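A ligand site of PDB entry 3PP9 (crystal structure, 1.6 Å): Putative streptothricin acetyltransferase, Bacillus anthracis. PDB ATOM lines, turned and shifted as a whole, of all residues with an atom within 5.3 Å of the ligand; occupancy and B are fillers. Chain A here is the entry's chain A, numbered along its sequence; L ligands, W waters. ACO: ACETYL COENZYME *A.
O2A of the ligand is in hydrogen-bond range of N of Lys 119 (2.8 Å).
NZ of Lys 119 lies within salt-bridge range of O7A of the ligand (2.5 Å).
N of Gly 118 is in hydrogen-bond range of O5A of the ligand.
The backbone NH (N) of Ile 106 lies within hydrogen-bond range of an oxygen (O) of the ligand, at 3.1 Å.
A nitrogen (N4P) of the ligand is in hydrogen-bond range of the backbone carbonyl oxygen (O) of Ile 106 (2.8 Å).
The backbone NH of Thr 114 lies within hydrogen-bond range of an oxygen (O4A) of the ligand.
O1A of the ligand sits at hydrogen-bond distance from N of Gly 116 (2.8 Å).
N of Val 108 lies within hydrogen-bond range of O9P of the ligand.
The side-chain amide nitrogen (ND2) of Asn 145 lies within hydrogen-bond range of an oxygen (O5P) of the ligand (3.0 Å).
The side-chain hydroxyl (OH) of Tyr 152 lies close to a sulfur (S1P) of the ligand (3.4 Å).
O1A of the ligand is in hydrogen-bond range of N of Leu 115 (3.3 Å).
The guanidinium group of Arg 113 lies close to an oxygen (O9P) of the ligand, 3.5 Å away.
NZ of Lys 154 is in salt-bridge range of O9A of the ligand (3.8 Å).
OG1 of Thr 141 lies close to S1P of the ligand, 3.8 Å away.
O of Asp 24 touches C7P of the ligand (3.8 Å).
CD1 of Phe 26 touches O5P of the ligand (3.9 Å).
CE1 of Tyr 57 touches C2P of the ligand, at 3.4 Å.
Ile 103 touches the ligand.
CA of Asp 105 touches O of the ligand, at 3.4 Å.
Thr 107 touches the ligand.
N of Val 117 touches O5A of the ligand, 3.6 Å away.
CB of Leu 139 touches CH3 of the ligand, 3.9 Å away.
Glu 140 touches the ligand.
Ala 147 touches the ligand.
Lys 150 touches the ligand (CB to C2A, 3.6 Å).
Phe 151 touches the ligand (CE1 to O3A, 3.5 Å).
Of the 31 residues printed, 24 come within 4 Å of the ligand.
Water W5 lies within hydrogen-bond range of an oxygen (O1A) of the ligand (2.8 Å), the backbone carbonyl oxygen of Thr 114 (3.3 Å) and the backbone NH of Gly 116 (3.4 Å).
Water W6 bridges OD1 of Asn 145 (2.8 Å) and O5P of the ligand (2.9 Å).
Water W8 lies within hydrogen-bond range of an oxygen (O2B) of the ligand (2.9 Å) and the backbone carbonyl oxygen of Thr 114 (3.1 Å).
Water W7 bridges NH1 of Arg 113 (3.3 Å) and OAP of the ligand (3.3 Å).
Water W10 bridges O of Ile 103 and N of Glu 140.
The backbone carbonyl oxygen of Val 108 is in hydrogen-bond range of the guanidinium group of Arg 113, at 2.8 Å.
The side-chain amide oxygen (OD1) of Asn 145 sits at hydrogen-bond distance from the backbone NH (N) of Ala 148 (3.2 Å).
The backbone carbonyl oxygen (O) of Ser 25 is in hydrogen-bond range of the guanidinium group (NH1) of Arg 113, at 2.7 Å.
OD1 of Asp 105 lies within hydrogen-bond range of OG1 of Thr 107 (2.8 Å).
O of Glu 104 is in hydrogen-bond range of OH of Tyr 57 (3.2 Å).
The side-chain sulfur (SG) of Cys 155 sits at hydrogen-bond distance from the backbone carbonyl oxygen (O) of Phe 151, at 3.4 Å.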
ATOM      1  N   ASP A  24      28.705  24.916  17.914  1.00  0.00           N
ATOM      2  CA  ASP A  24      29.264  25.256  19.238  1.00  0.00           C
ATOM      3  C   ASP A  24      30.433  26.217  19.096  1.00  0.00           C
ATOM      4  O   ASP A  24      31.182  26.424  20.063  1.00  0.00           O
ATOM      5  CB  ASP A  24      29.705  24.028  20.082  1.00  0.00           C
ATOM      6  CG  ASP A  24      30.969  23.335  19.570  1.00  0.00           C
ATOM      7  OD1 ASP A  24      31.448  23.658  18.469  1.00  0.00           O
ATOM      8  OD2 ASP A  24      31.498  22.440  20.281  1.00  0.00           O
ATOM      9  N   SER A  25      30.612  26.818  17.926  1.00  0.00           N
ATOM     10  CA  SER A  25      31.692  27.772  17.760  1.00  0.00           C
ATOM     11  C   SER A  25      31.341  29.085  18.417  1.00  0.00           C
ATOM     12  O   SER A  25      30.173  29.429  18.616  1.00  0.00           O
ATOM     13  CB  SER A  25      32.031  27.994  16.268  1.00  0.00           C
ATOM     14  OG  SER A  25      30.998  28.677  15.568  1.00  0.00           O
ATOM     15  N   PHE A  26      32.396  29.838  18.753  1.00  0.00           N
ATOM     16  CA  PHE A  26      32.226  31.139  19.366  1.00  0.00           C
ATOM     17  C   PHE A  26      33.383  32.033  18.970  1.00  0.00           C
ATOM     18  O   PHE A  26      34.403  31.575  18.460  1.00  0.00           O
ATOM     19  CB  PHE A  26      32.097  31.049  20.882  1.00  0.00           C
ATOM     20  CG  PHE A  26      33.265  30.405  21.563  1.00  0.00           C
ATOM     21  CD1 PHE A  26      33.320  29.020  21.691  1.00  0.00           C
ATOM     22  CD2 PHE A  26      34.280  31.168  22.113  1.00  0.00           C
ATOM     23  CE1 PHE A  26      34.378  28.402  22.337  1.00  0.00           C
ATOM     24  CE2 PHE A  26      35.340  30.558  22.763  1.00  0.00           C
ATOM     25  CZ  PHE A  26      35.393  29.177  22.849  1.00  0.00           C
ATOM     26  N   TYR A  57      34.293  24.870  20.576  1.00  0.00           N
ATOM     27  CA  TYR A  57      34.585  24.422  21.915  1.00  0.00           C
ATOM     28  C   TYR A  57      35.205  23.016  21.871  1.00  0.00           C
ATOM     29  O   TYR A  57      36.211  22.744  22.526  1.00  0.00           O
ATOM     30  CB  TYR A  57      33.332  24.422  22.780  1.00  0.00           C
ATOM     31  CG  TYR A  57      33.623  23.832  24.114  1.00  0.00           C
ATOM     32  CD1 TYR A  57      34.481  24.463  24.988  1.00  0.00           C
ATOM     33  CD2 TYR A  57      33.021  22.647  24.534  1.00  0.00           C
ATOM     34  CE1 TYR A  57      34.765  23.920  26.223  1.00  0.00           C
ATOM     35  CE2 TYR A  57      33.299  22.119  25.763  1.00  0.00           C
ATOM     36  CZ  TYR A  57      34.166  22.757  26.607  1.00  0.00           C
ATOM     37  OH  TYR A  57      34.451  22.246  27.842  1.00  0.00           O
ATOM     38  N   ILE A 103      30.360  20.077  34.859  1.00  0.00           N
ATOM     39  CA  ILE A 103      29.860  20.320  33.515  1.00  0.00           C
ATOM     40  C   ILE A 103      30.981  20.063  32.524  1.00  0.00           C
ATOM     41  O   ILE A 103      31.939  20.831  32.444  1.00  0.00           O
ATOM     42  CB  ILE A 103      29.355  21.759  33.339  1.00  0.00           C
ATOM     43  CG1 ILE A 103      28.276  22.116  34.353  1.00  0.00           C
ATOM     44  CG2 ILE A 103      28.878  21.946  31.872  1.00  0.00           C
ATOM     45  CD1 ILE A 103      27.836  23.591  34.305  1.00  0.00           C
ATOM     46  N   GLU A 104      30.858  18.983  31.771  1.00  0.00           N
ATOM     47  CA  GLU A 104      31.832  18.621  30.777  1.00  0.00           C
ATOM     48  C   GLU A 104      31.689  19.495  29.536  1.00  0.00           C
ATOM     49  O   GLU A 104      32.701  19.786  28.869  1.00  0.00           O
ATOM     50  CB  GLU A 104      31.641  17.178  30.358  1.00  0.00           C
ATOM     51  CG  GLU A 104      31.972  16.172  31.442  1.00  0.00           C
ATOM     52  CD  GLU A 104      33.449  15.988  31.686  1.00  0.00           C
ATOM     53  OE1 GLU A 104      34.281  16.542  30.936  1.00  0.00           O
ATOM     54  OE2 GLU A 104      33.786  15.285  32.647  1.00  0.00           O
ATOM     55  N   ASP A 105      30.450  19.894  29.237  1.00  0.00           N
ATOM     56  CA  ASP A 105      30.145  20.729  28.076  1.00  0.00           C
ATOM     57  C   ASP A 105      28.745  21.270  28.180  1.00  0.00           C
ATOM     58  O   ASP A 105      27.830  20.546  28.590  1.00  0.00           O
ATOM     59  CB  ASP A 105      30.259  19.864  26.796  1.00  0.00           C
ATOM     60  CG  ASP A 105      29.986  20.611  25.470  1.00  0.00           C
ATOM     61  OD1 ASP A 105      29.436  21.716  25.448  1.00  0.00           O
ATOM     62  OD2 ASP A 105      30.309  19.997  24.389  1.00  0.00           O
ATOM     63  N   ILE A 106      28.604  22.556  27.904  1.00  0.00           N
ATOM     64  CA  ILE A 106      27.291  23.172  27.791  1.00  0.00           C
ATOM     65  C   ILE A 106      27.372  23.914  26.456  1.00  0.00           C
ATOM     66  O   ILE A 106      28.310  24.668  26.203  1.00  0.00           O
ATOM     67  CB  ILE A 106      26.849  24.064  28.951  1.00  0.00           C
ATOM     68  CG1 ILE A 106      25.449  24.659  28.652  1.00  0.00           C
ATOM     69  CG2 ILE A 106      27.868  25.200  29.234  1.00  0.00           C
ATOM     70  CD1 ILE A 106      24.866  25.516  29.759  1.00  0.00           C
ATOM     71  N   THR A 107      26.395  23.649  25.595  1.00  0.00           N
ATOM     72  CA  THR A 107      26.356  24.299  24.292  1.00  0.00           C
ATOM     73  C   THR A 107      24.942  24.666  23.897  1.00  0.00           C
ATOM     74  O   THR A 107      24.034  23.875  24.033  1.00  0.00           O
ATOM     75  CB  THR A 107      26.896  23.402  23.183  1.00  0.00           C
ATOM     76  OG1 THR A 107      28.301  23.175  23.360  1.00  0.00           O
ATOM     77  CG2 THR A 107      26.700  24.045  21.792  1.00  0.00           C
ATOM     78  N   VAL A 108      24.788  25.898  23.425  1.00  0.00           N
ATOM     79  CA  VAL A 108      23.542  26.357  22.851  1.00  0.00           C
ATOM     80  C   VAL A 108      23.911  26.703  21.388  1.00  0.00           C
ATOM     81  O   VAL A 108      24.917  27.373  21.119  1.00  0.00           O
ATOM     82  CB  VAL A 108      22.926  27.563  23.597  1.00  0.00           C
ATOM     83  CG1 VAL A 108      21.772  28.185  22.803  1.00  0.00           C
ATOM     84  CG2 VAL A 108      22.458  27.120  24.985  1.00  0.00           C
ATOM     85  N   TYR A 112      20.761  30.677  18.550  1.00  0.00           N
ATOM     86  CA  TYR A 112      19.823  30.851  19.641  1.00  0.00           C
ATOM     87  C   TYR A 112      20.405  31.379  20.943  1.00  0.00           C
ATOM     88  O   TYR A 112      19.717  31.391  21.973  1.00  0.00           O
ATOM     89  CB  TYR A 112      19.107  29.533  19.943  1.00  0.00           C
ATOM     90  CG  TYR A 112      18.269  29.013  18.811  1.00  0.00           C
ATOM     91  CD1 TYR A 112      17.050  29.575  18.534  1.00  0.00           C
ATOM     92  CD2 TYR A 112      18.691  27.943  18.013  1.00  0.00           C
ATOM     93  CE1 TYR A 112      16.271  29.115  17.495  1.00  0.00           C
ATOM     94  CE2 TYR A 112      17.909  27.477  16.962  1.00  0.00           C
ATOM     95  CZ  TYR A 112      16.701  28.069  16.716  1.00  0.00           C
ATOM     96  OH  TYR A 112      15.890  27.642  15.677  1.00  0.00           O
ATOM     97  N   ARG A 113      21.668  31.779  20.934  1.00  0.00           N
ATOM     98  CA  ARG A 113      22.290  32.283  22.165  1.00  0.00           C
ATOM     99  C   ARG A 113      21.774  33.642  22.583  1.00  0.00           C
ATOM    100  O   ARG A 113      21.298  34.429  21.774  1.00  0.00           O
ATOM    101  CB  ARG A 113      23.790  32.332  22.012  1.00  0.00           C
ATOM    102  CG  ARG A 113      24.421  30.964  21.844  1.00  0.00           C
ATOM    103  CD  ARG A 113      25.918  31.049  21.650  1.00  0.00           C
ATOM    104  NE  ARG A 113      26.409  29.788  21.095  1.00  0.00           N
ATOM    105  CZ  ARG A 113      27.541  29.640  20.434  1.00  0.00           C
ATOM    106  NH1 ARG A 113      28.370  30.663  20.279  1.00  0.00           N
ATOM    107  NH2 ARG A 113      27.819  28.467  19.896  1.00  0.00           N
ATOM    108  N   THR A 114      21.927  33.892  23.886  1.00  0.00           N
ATOM    109  CA  THR A 114      21.542  35.102  24.624  1.00  0.00           C
ATOM    110  C   THR A 114      20.016  35.227  24.844  1.00  0.00           C
ATOM    111  O   THR A 114      19.526  36.296  25.242  1.00  0.00           O
ATOM    112  CB  THR A 114      22.075  36.405  23.980  1.00  0.00           C
ATOM    113  OG1 THR A 114      21.318  36.779  22.834  1.00  0.00           O
ATOM    114  CG2 THR A 114      23.574  36.263  23.638  1.00  0.00           C
ATOM    115  N   LEU A 115      19.306  34.128  24.608  1.00  0.00           N
ATOM    116  CA  LEU A 115      17.851  34.055  24.753  1.00  0.00           C
ATOM    117  C   LEU A 115      17.388  33.201  25.944  1.00  0.00           C
ATOM    118  O   LEU A 115      16.216  32.804  26.017  1.00  0.00           O
ATOM    119  CB  LEU A 115      17.237  33.531  23.442  1.00  0.00           C
ATOM    120  CG  LEU A 115      17.491  34.428  22.232  1.00  0.00           C
ATOM    121  CD1 LEU A 115      16.983  33.760  20.949  1.00  0.00           C
ATOM    122  CD2 LEU A 115      16.892  35.833  22.392  1.00  0.00           C
ATOM    123  N   GLY A 116      18.291  32.955  26.890  1.00  0.00           N
ATOM    124  CA  GLY A 116      17.997  32.231  28.114  1.00  0.00           C
ATOM    125  C   GLY A 116      18.045  30.712  28.156  1.00  0.00           C
ATOM    126  O   GLY A 116      17.779  30.105  29.198  1.00  0.00           O
ATOM    127  N   VAL A 117      18.385  30.096  27.032  1.00  0.00           N
ATOM    128  CA  VAL A 117      18.434  28.644  26.969  1.00  0.00           C
ATOM    129  C   VAL A 117      19.516  28.059  27.891  1.00  0.00           C
ATOM    130  O   VAL A 117      19.284  27.097  28.638  1.00  0.00           O
ATOM    131  CB  VAL A 117      18.605  28.158  25.519  1.00  0.00           C
ATOM    132  CG1 VAL A 117      18.689  26.639  25.487  1.00  0.00           C
ATOM    133  CG2 VAL A 117      17.460  28.623  24.653  1.00  0.00           C
ATOM    134  N   GLY A 118      20.691  28.661  27.863  1.00  0.00           N
ATOM    135  CA  GLY A 118      21.789  28.216  28.714  1.00  0.00           C
ATOM    136  C   GLY A 118      21.430  28.246  30.194  1.00  0.00           C
ATOM    137  O   GLY A 118      21.729  27.306  30.941  1.00  0.00           O
ATOM    138  N   LYS A 119      20.804  29.335  30.639  1.00  0.00           N
ATOM    139  CA  LYS A 119      20.404  29.426  32.044  1.00  0.00           C
ATOM    140  C   LYS A 119      19.447  28.294  32.426  1.00  0.00           C
ATOM    141  O   LYS A 119      19.499  27.775  33.551  1.00  0.00           O
ATOM    142  CB  LYS A 119      19.760  30.781  32.334  1.00  0.00           C
ATOM    143  CG  LYS A 119      19.324  30.946  33.784  1.00  0.00           C
ATOM    144  CD  LYS A 119      18.673  32.325  34.040  1.00  0.00           C
ATOM    145  CE  LYS A 119      19.653  33.474  33.852  1.00  0.00           C
ATOM    146  NZ  LYS A 119      19.036  34.783  34.254  1.00  0.00           N
ATOM    147  N   ARG A 120      18.545  27.946  31.507  1.00  0.00           N
ATOM    148  CA  ARG A 120      17.586  26.845  31.763  1.00  0.00           C
ATOM    149  C   ARG A 120      18.324  25.509  31.858  1.00  0.00           C
ATOM    150  O   ARG A 120      17.957  24.644  32.647  1.00  0.00           O
ATOM    151  CB  ARG A 120      16.504  26.788  30.675  1.00  0.00           C
ATOM    152  CG  ARG A 120      15.467  27.887  30.731  1.00  0.00           C
ATOM    153  CD  ARG A 120      14.441  27.595  31.818  1.00  0.00           C
ATOM    154  NE  ARG A 120      13.759  26.325  31.536  1.00  0.00           N
ATOM    155  CZ  ARG A 120      12.698  26.175  30.744  1.00  0.00           C
ATOM    156  NH1 ARG A 120      12.130  27.222  30.145  1.00  0.00           N
ATOM    157  NH2 ARG A 120      12.178  24.964  30.556  1.00  0.00           N
ATOM    158  N   LEU A 139      33.070  23.606  36.900  1.00  0.00           N
ATOM    159  CA  LEU A 139      33.503  23.407  35.523  1.00  0.00           C
ATOM    160  C   LEU A 139      34.802  24.135  35.286  1.00  0.00           C
ATOM    161  O   LEU A 139      35.295  24.846  36.152  1.00  0.00           O
ATOM    162  CB  LEU A 139      32.413  23.880  34.545  1.00  0.00           C
ATOM    163  CG  LEU A 139      31.945  25.343  34.461  1.00  0.00           C
ATOM    164  CD1 LEU A 139      31.210  25.805  35.680  1.00  0.00           C
ATOM    165  CD2 LEU A 139      33.046  26.335  34.056  1.00  0.00           C
ATOM    166  N   GLU A 140      35.406  23.849  34.134  1.00  0.00           N
ATOM    167  CA  GLU A 140      36.642  24.493  33.711  1.00  0.00           C
ATOM    168  C   GLU A 140      36.357  25.134  32.382  1.00  0.00           C
ATOM    169  O   GLU A 140      35.605  24.591  31.569  1.00  0.00           O
ATOM    170  CB  GLU A 140      37.781  23.494  33.519  1.00  0.00           C
ATOM    171  CG  GLU A 140      39.116  24.108  33.023  1.00  0.00           C
ATOM    172  CD  GLU A 140      39.172  24.471  31.522  1.00  0.00           C
ATOM    173  OE1 GLU A 140      38.223  24.166  30.754  1.00  0.00           O
ATOM    174  OE2 GLU A 140      40.203  25.032  31.091  1.00  0.00           O
ATOM    175  N   THR A 141      36.926  26.310  32.191  1.00  0.00           N
ATOM    176  CA  THR A 141      36.816  27.022  30.939  1.00  0.00           C
ATOM    177  C   THR A 141      38.201  27.673  30.750  1.00  0.00           C
ATOM    178  O   THR A 141      39.073  27.521  31.611  1.00  0.00           O
ATOM    179  CB  THR A 141      35.552  27.962  30.868  1.00  0.00           C
ATOM    180  OG1 THR A 141      35.397  28.514  29.543  1.00  0.00           O
ATOM    181  CG2 THR A 141      35.601  29.057  31.920  1.00  0.00           C
ATOM    182  N   ASN A 145      37.569  32.547  26.791  1.00  0.00           N
ATOM    183  CA  ASN A 145      36.141  32.379  26.527  1.00  0.00           C
ATOM    184  C   ASN A 145      35.400  33.317  27.480  1.00  0.00           C
ATOM    185  O   ASN A 145      34.772  32.890  28.441  1.00  0.00           O
ATOM    186  CB  ASN A 145      35.722  30.937  26.706  1.00  0.00           C
ATOM    187  CG  ASN A 145      34.347  30.642  26.170  1.00  0.00           C
ATOM    188  OD1 ASN A 145      33.588  31.567  25.835  1.00  0.00           O
ATOM    189  ND2 ASN A 145      34.027  29.342  26.049  1.00  0.00           N
ATOM    190  N   VAL A 146      35.506  34.621  27.200  1.00  0.00           N
ATOM    191  CA  VAL A 146      34.885  35.642  28.045  1.00  0.00           C
ATOM    192  C   VAL A 146      33.356  35.510  28.044  1.00  0.00           C
ATOM    193  O   VAL A 146      32.728  35.686  29.086  1.00  0.00           O
ATOM    194  CB  VAL A 146      35.395  37.061  27.679  1.00  0.00           C
ATOM    195  CG1 VAL A 146      34.672  38.132  28.507  1.00  0.00           C
ATOM    196  CG2 VAL A 146      36.909  37.149  27.897  1.00  0.00           C
ATOM    197  N   ALA A 147      32.766  35.114  26.922  1.00  0.00           N
ATOM    198  CA  ALA A 147      31.314  34.947  26.848  1.00  0.00           C
ATOM    199  C   ALA A 147      30.883  33.928  27.901  1.00  0.00           C
ATOM    200  O   ALA A 147      29.942  34.159  28.654  1.00  0.00           O
ATOM    201  CB  ALA A 147      30.874  34.461  25.477  1.00  0.00           C
ATOM    202  N   ALA A 148      31.556  32.782  27.921  1.00  0.00           N
ATOM    203  CA  ALA A 148      31.240  31.720  28.888  1.00  0.00           C
ATOM    204  C   ALA A 148      31.503  32.187  30.325  1.00  0.00           C
ATOM    205  O   ALA A 148      30.699  31.925  31.233  1.00  0.00           O
ATOM    206  CB  ALA A 148      32.042  30.470  28.591  1.00  0.00           C
ATOM    207  N   LYS A 150      31.388  35.245  31.584  1.00  0.00           N
ATOM    208  CA  LYS A 150      30.321  36.168  32.003  1.00  0.00           C
ATOM    209  C   LYS A 150      29.032  35.400  32.250  1.00  0.00           C
ATOM    210  O   LYS A 150      28.299  35.711  33.187  1.00  0.00           O
ATOM    211  CB  LYS A 150      30.125  37.260  30.959  1.00  0.00           C
ATOM    212  CG  LYS A 150      31.289  38.232  30.852  1.00  0.00           C
ATOM    213  CD  LYS A 150      31.441  39.040  32.137  1.00  0.00           C
ATOM    214  CE  LYS A 150      32.583  40.043  32.029  1.00  0.00           C
ATOM    215  NZ  LYS A 150      32.682  40.908  33.227  1.00  0.00           N
ATOM    216  N   PHE A 151      28.750  34.408  31.420  1.00  0.00           N
ATOM    217  CA  PHE A 151      27.561  33.580  31.583  1.00  0.00           C
ATOM    218  C   PHE A 151      27.594  32.857  32.947  1.00  0.00           C
ATOM    219  O   PHE A 151      26.617  32.897  33.711  1.00  0.00           O
ATOM    220  CB  PHE A 151      27.502  32.545  30.457  1.00  0.00           C
ATOM    221  CG  PHE A 151      26.493  31.429  30.676  1.00  0.00           C
ATOM    222  CD1 PHE A 151      25.144  31.653  30.550  1.00  0.00           C
ATOM    223  CD2 PHE A 151      26.921  30.151  30.977  1.00  0.00           C
ATOM    224  CE1 PHE A 151      24.245  30.626  30.757  1.00  0.00           C
ATOM    225  CE2 PHE A 151      26.019  29.114  31.181  1.00  0.00           C
ATOM    226  CZ  PHE A 151      24.673  29.347  31.058  1.00  0.00           C
ATOM    227  N   TYR A 152      28.709  32.212  33.280  1.00  0.00           N
ATOM    228  CA  TYR A 152      28.808  31.520  34.581  1.00  0.00           C
ATOM    229  C   TYR A 152      28.659  32.513  35.745  1.00  0.00           C
ATOM    230  O   TYR A 152      28.016  32.194  36.762  1.00  0.00           O
ATOM    231  CB  TYR A 152      30.084  30.674  34.692  1.00  0.00           C
ATOM    232  CG  TYR A 152      30.129  29.571  33.671  1.00  0.00           C
ATOM    233  CD1 TYR A 152      29.159  28.590  33.639  1.00  0.00           C
ATOM    234  CD2 TYR A 152      31.193  29.475  32.784  1.00  0.00           C
ATOM    235  CE1 TYR A 152      29.205  27.574  32.688  1.00  0.00           C
ATOM    236  CE2 TYR A 152      31.233  28.465  31.855  1.00  0.00           C
ATOM    237  CZ  TYR A 152      30.250  27.514  31.813  1.00  0.00           C
ATOM    238  OH  TYR A 152      30.286  26.500  30.862  1.00  0.00           O
ATOM    239  N   LYS A 154      26.948  35.275  35.781  1.00  0.00           N
ATOM    240  CA  LYS A 154      25.529  35.623  35.854  1.00  0.00           C
ATOM    241  C   LYS A 154      24.708  34.512  36.507  1.00  0.00           C
ATOM    242  O   LYS A 154      23.685  34.779  37.165  1.00  0.00           O
ATOM    243  CB  LYS A 154      24.948  35.959  34.476  1.00  0.00           C
ATOM    244  CG  LYS A 154      25.306  37.314  33.921  1.00  0.00           C
ATOM    245  CD  LYS A 154      24.678  38.420  34.750  1.00  0.00           C
ATOM    246  CE  LYS A 154      24.951  39.786  34.146  1.00  0.00           C
ATOM    247  NZ  LYS A 154      24.386  40.853  34.995  1.00  0.00           N
ATOM    248  N   CYS A 155      25.169  33.271  36.358  1.00  0.00           N
ATOM    249  CA  CYS A 155      24.521  32.096  36.928  1.00  0.00           C
ATOM    250  C   CYS A 155      24.906  31.851  38.396  1.00  0.00           C
ATOM    251  O   CYS A 155      24.438  30.880  39.003  1.00  0.00           O
ATOM    252  CB  CYS A 155      24.790  30.853  36.072  1.00  0.00           C
ATOM    253  SG  CYS A 155      23.989  30.874  34.464  1.00  0.00           S
HETATM  254  N1A ACO L   1      28.514  38.054  27.242  1.00  0.00           N
HETATM  255  C2A ACO L   1      28.007  38.528  28.392  1.00  0.00           C
HETATM  256  N3A ACO L   1      26.999  37.942  29.047  1.00  0.00           N
HETATM  257  C4A ACO L   1      26.435  36.814  28.549  1.00  0.00           C
HETATM  258  C5A ACO L   1      26.927  36.259  27.288  1.00  0.00           C
HETATM  259  C6A ACO L   1      28.020  36.952  26.627  1.00  0.00           C
HETATM  260  N6A ACO L   1      28.501  36.467  25.463  1.00  0.00           N
HETATM  261  N7A ACO L   1      26.195  35.165  27.022  1.00  0.00           N
HETATM  262  C8A ACO L   1      25.304  35.033  28.024  1.00  0.00           C
HETATM  263  N9A ACO L   1      25.451  36.010  28.933  1.00  0.00           N
HETATM  264  C1B ACO L   1      24.635  36.239  30.138  1.00  0.00           C
HETATM  265  C2B ACO L   1      23.264  36.740  29.661  1.00  0.00           C
HETATM  266  O2B ACO L   1      23.181  38.144  29.402  1.00  0.00           O
HETATM  267  C3B ACO L   1      22.340  36.299  30.763  1.00  0.00           C
HETATM  268  O3B ACO L   1      22.344  37.289  31.779  1.00  0.00           O
HETATM  269  P3B ACO L   1      21.014  37.753  32.552  1.00  0.00           P
HETATM  270  O7A ACO L   1      20.533  36.498  33.266  1.00  0.00           O
HETATM  271  O8A ACO L   1      20.109  38.217  31.446  1.00  0.00           O
HETATM  272  O9A ACO L   1      21.539  38.834  33.466  1.00  0.00           O
HETATM  273  C4B ACO L   1      22.991  35.028  31.289  1.00  0.00           C
HETATM  274  O4B ACO L   1      24.373  35.071  30.902  1.00  0.00           O
HETATM  275  C5B ACO L   1      22.305  33.796  30.725  1.00  0.00           C
HETATM  276  O5B ACO L   1      22.584  33.722  29.325  1.00  0.00           O
HETATM  277  P1A ACO L   1      21.789  32.694  28.385  1.00  0.00           P
HETATM  278  O1A ACO L   1      21.063  33.465  27.306  1.00  0.00           O
HETATM  279  O2A ACO L   1      21.026  31.771  29.278  1.00  0.00           O
HETATM  280  O3A ACO L   1      23.059  31.923  27.732  1.00  0.00           O
HETATM  281  P2A ACO L   1      23.091  31.134  26.339  1.00  0.00           P
HETATM  282  O4A ACO L   1      23.617  32.132  25.353  1.00  0.00           O
HETATM  283  O5A ACO L   1      21.808  30.410  26.042  1.00  0.00           O
HETATM  284  O6A ACO L   1      24.182  29.973  26.620  1.00  0.00           O
HETATM  285  CBP ACO L   1      26.507  29.385  26.465  1.00  0.00           C
HETATM  286  CCP ACO L   1      25.473  30.270  27.136  1.00  0.00           C
HETATM  287  CDP ACO L   1      27.857  29.623  27.130  1.00  0.00           C
HETATM  288  CEP ACO L   1      26.098  27.918  26.605  1.00  0.00           C
HETATM  289  CAP ACO L   1      26.601  29.733  24.970  1.00  0.00           C
HETATM  290  OAP ACO L   1      27.202  31.043  24.812  1.00  0.00           O
HETATM  291  C9P ACO L   1      27.423  28.774  24.169  1.00  0.00           C
HETATM  292  O9P ACO L   1      26.983  27.707  23.797  1.00  0.00           O
HETATM  293  N8P ACO L   1      28.681  29.114  23.846  1.00  0.00           N
HETATM  294  C7P ACO L   1      29.549  28.282  23.013  1.00  0.00           C
HETATM  295  C6P ACO L   1      29.979  27.004  23.683  1.00  0.00           C
HETATM  296  C5P ACO L   1      30.679  27.331  24.972  1.00  0.00           C
HETATM  297  O5P ACO L   1      31.469  28.255  25.057  1.00  0.00           O
HETATM  298  N4P ACO L   1      30.390  26.579  26.008  1.00  0.00           N
HETATM  299  C3P ACO L   1      30.980  26.745  27.328  1.00  0.00           C
HETATM  300  C2P ACO L   1      32.359  26.083  27.279  1.00  0.00           C
HETATM  301  S1P ACO L   1      32.975  25.718  28.911  1.00  0.00           S
HETATM  302  C   ACO L   1      32.126  24.313  29.310  1.00  0.00           C
HETATM  303  O   ACO L   1      31.306  23.844  28.541  1.00  0.00           O
HETATM  304  CH3 ACO L   1      32.386  23.663  30.625  1.00  0.00           C
HETATM  305  O   HOH W   1      26.393  39.730  31.308  1.00  0.00           O
HETATM  306  O   HOH W   2      30.582  37.929  24.249  1.00  0.00           O
HETATM  307  O   HOH W   3      19.706  31.211  24.617  1.00  0.00           O
HETATM  308  O   HOH W   4      25.910  33.315  25.081  1.00  0.00           O
HETATM  309  O   HOH W   5      19.652  35.580  28.512  1.00  0.00           O
HETATM  310  O   HOH W   6      31.204  31.040  24.438  1.00  0.00           O
HETATM  311  O   HOH W   7      29.458  32.423  22.795  1.00  0.00           O
HETATM  312  O   HOH W   8      21.054  37.727  27.475  1.00  0.00           O
HETATM  313  O   HOH W   9      27.418  34.434  23.205  1.00  0.00           O
HETATM  314  O   HOH W  10      34.554  21.672  32.346  1.00  0.00           O
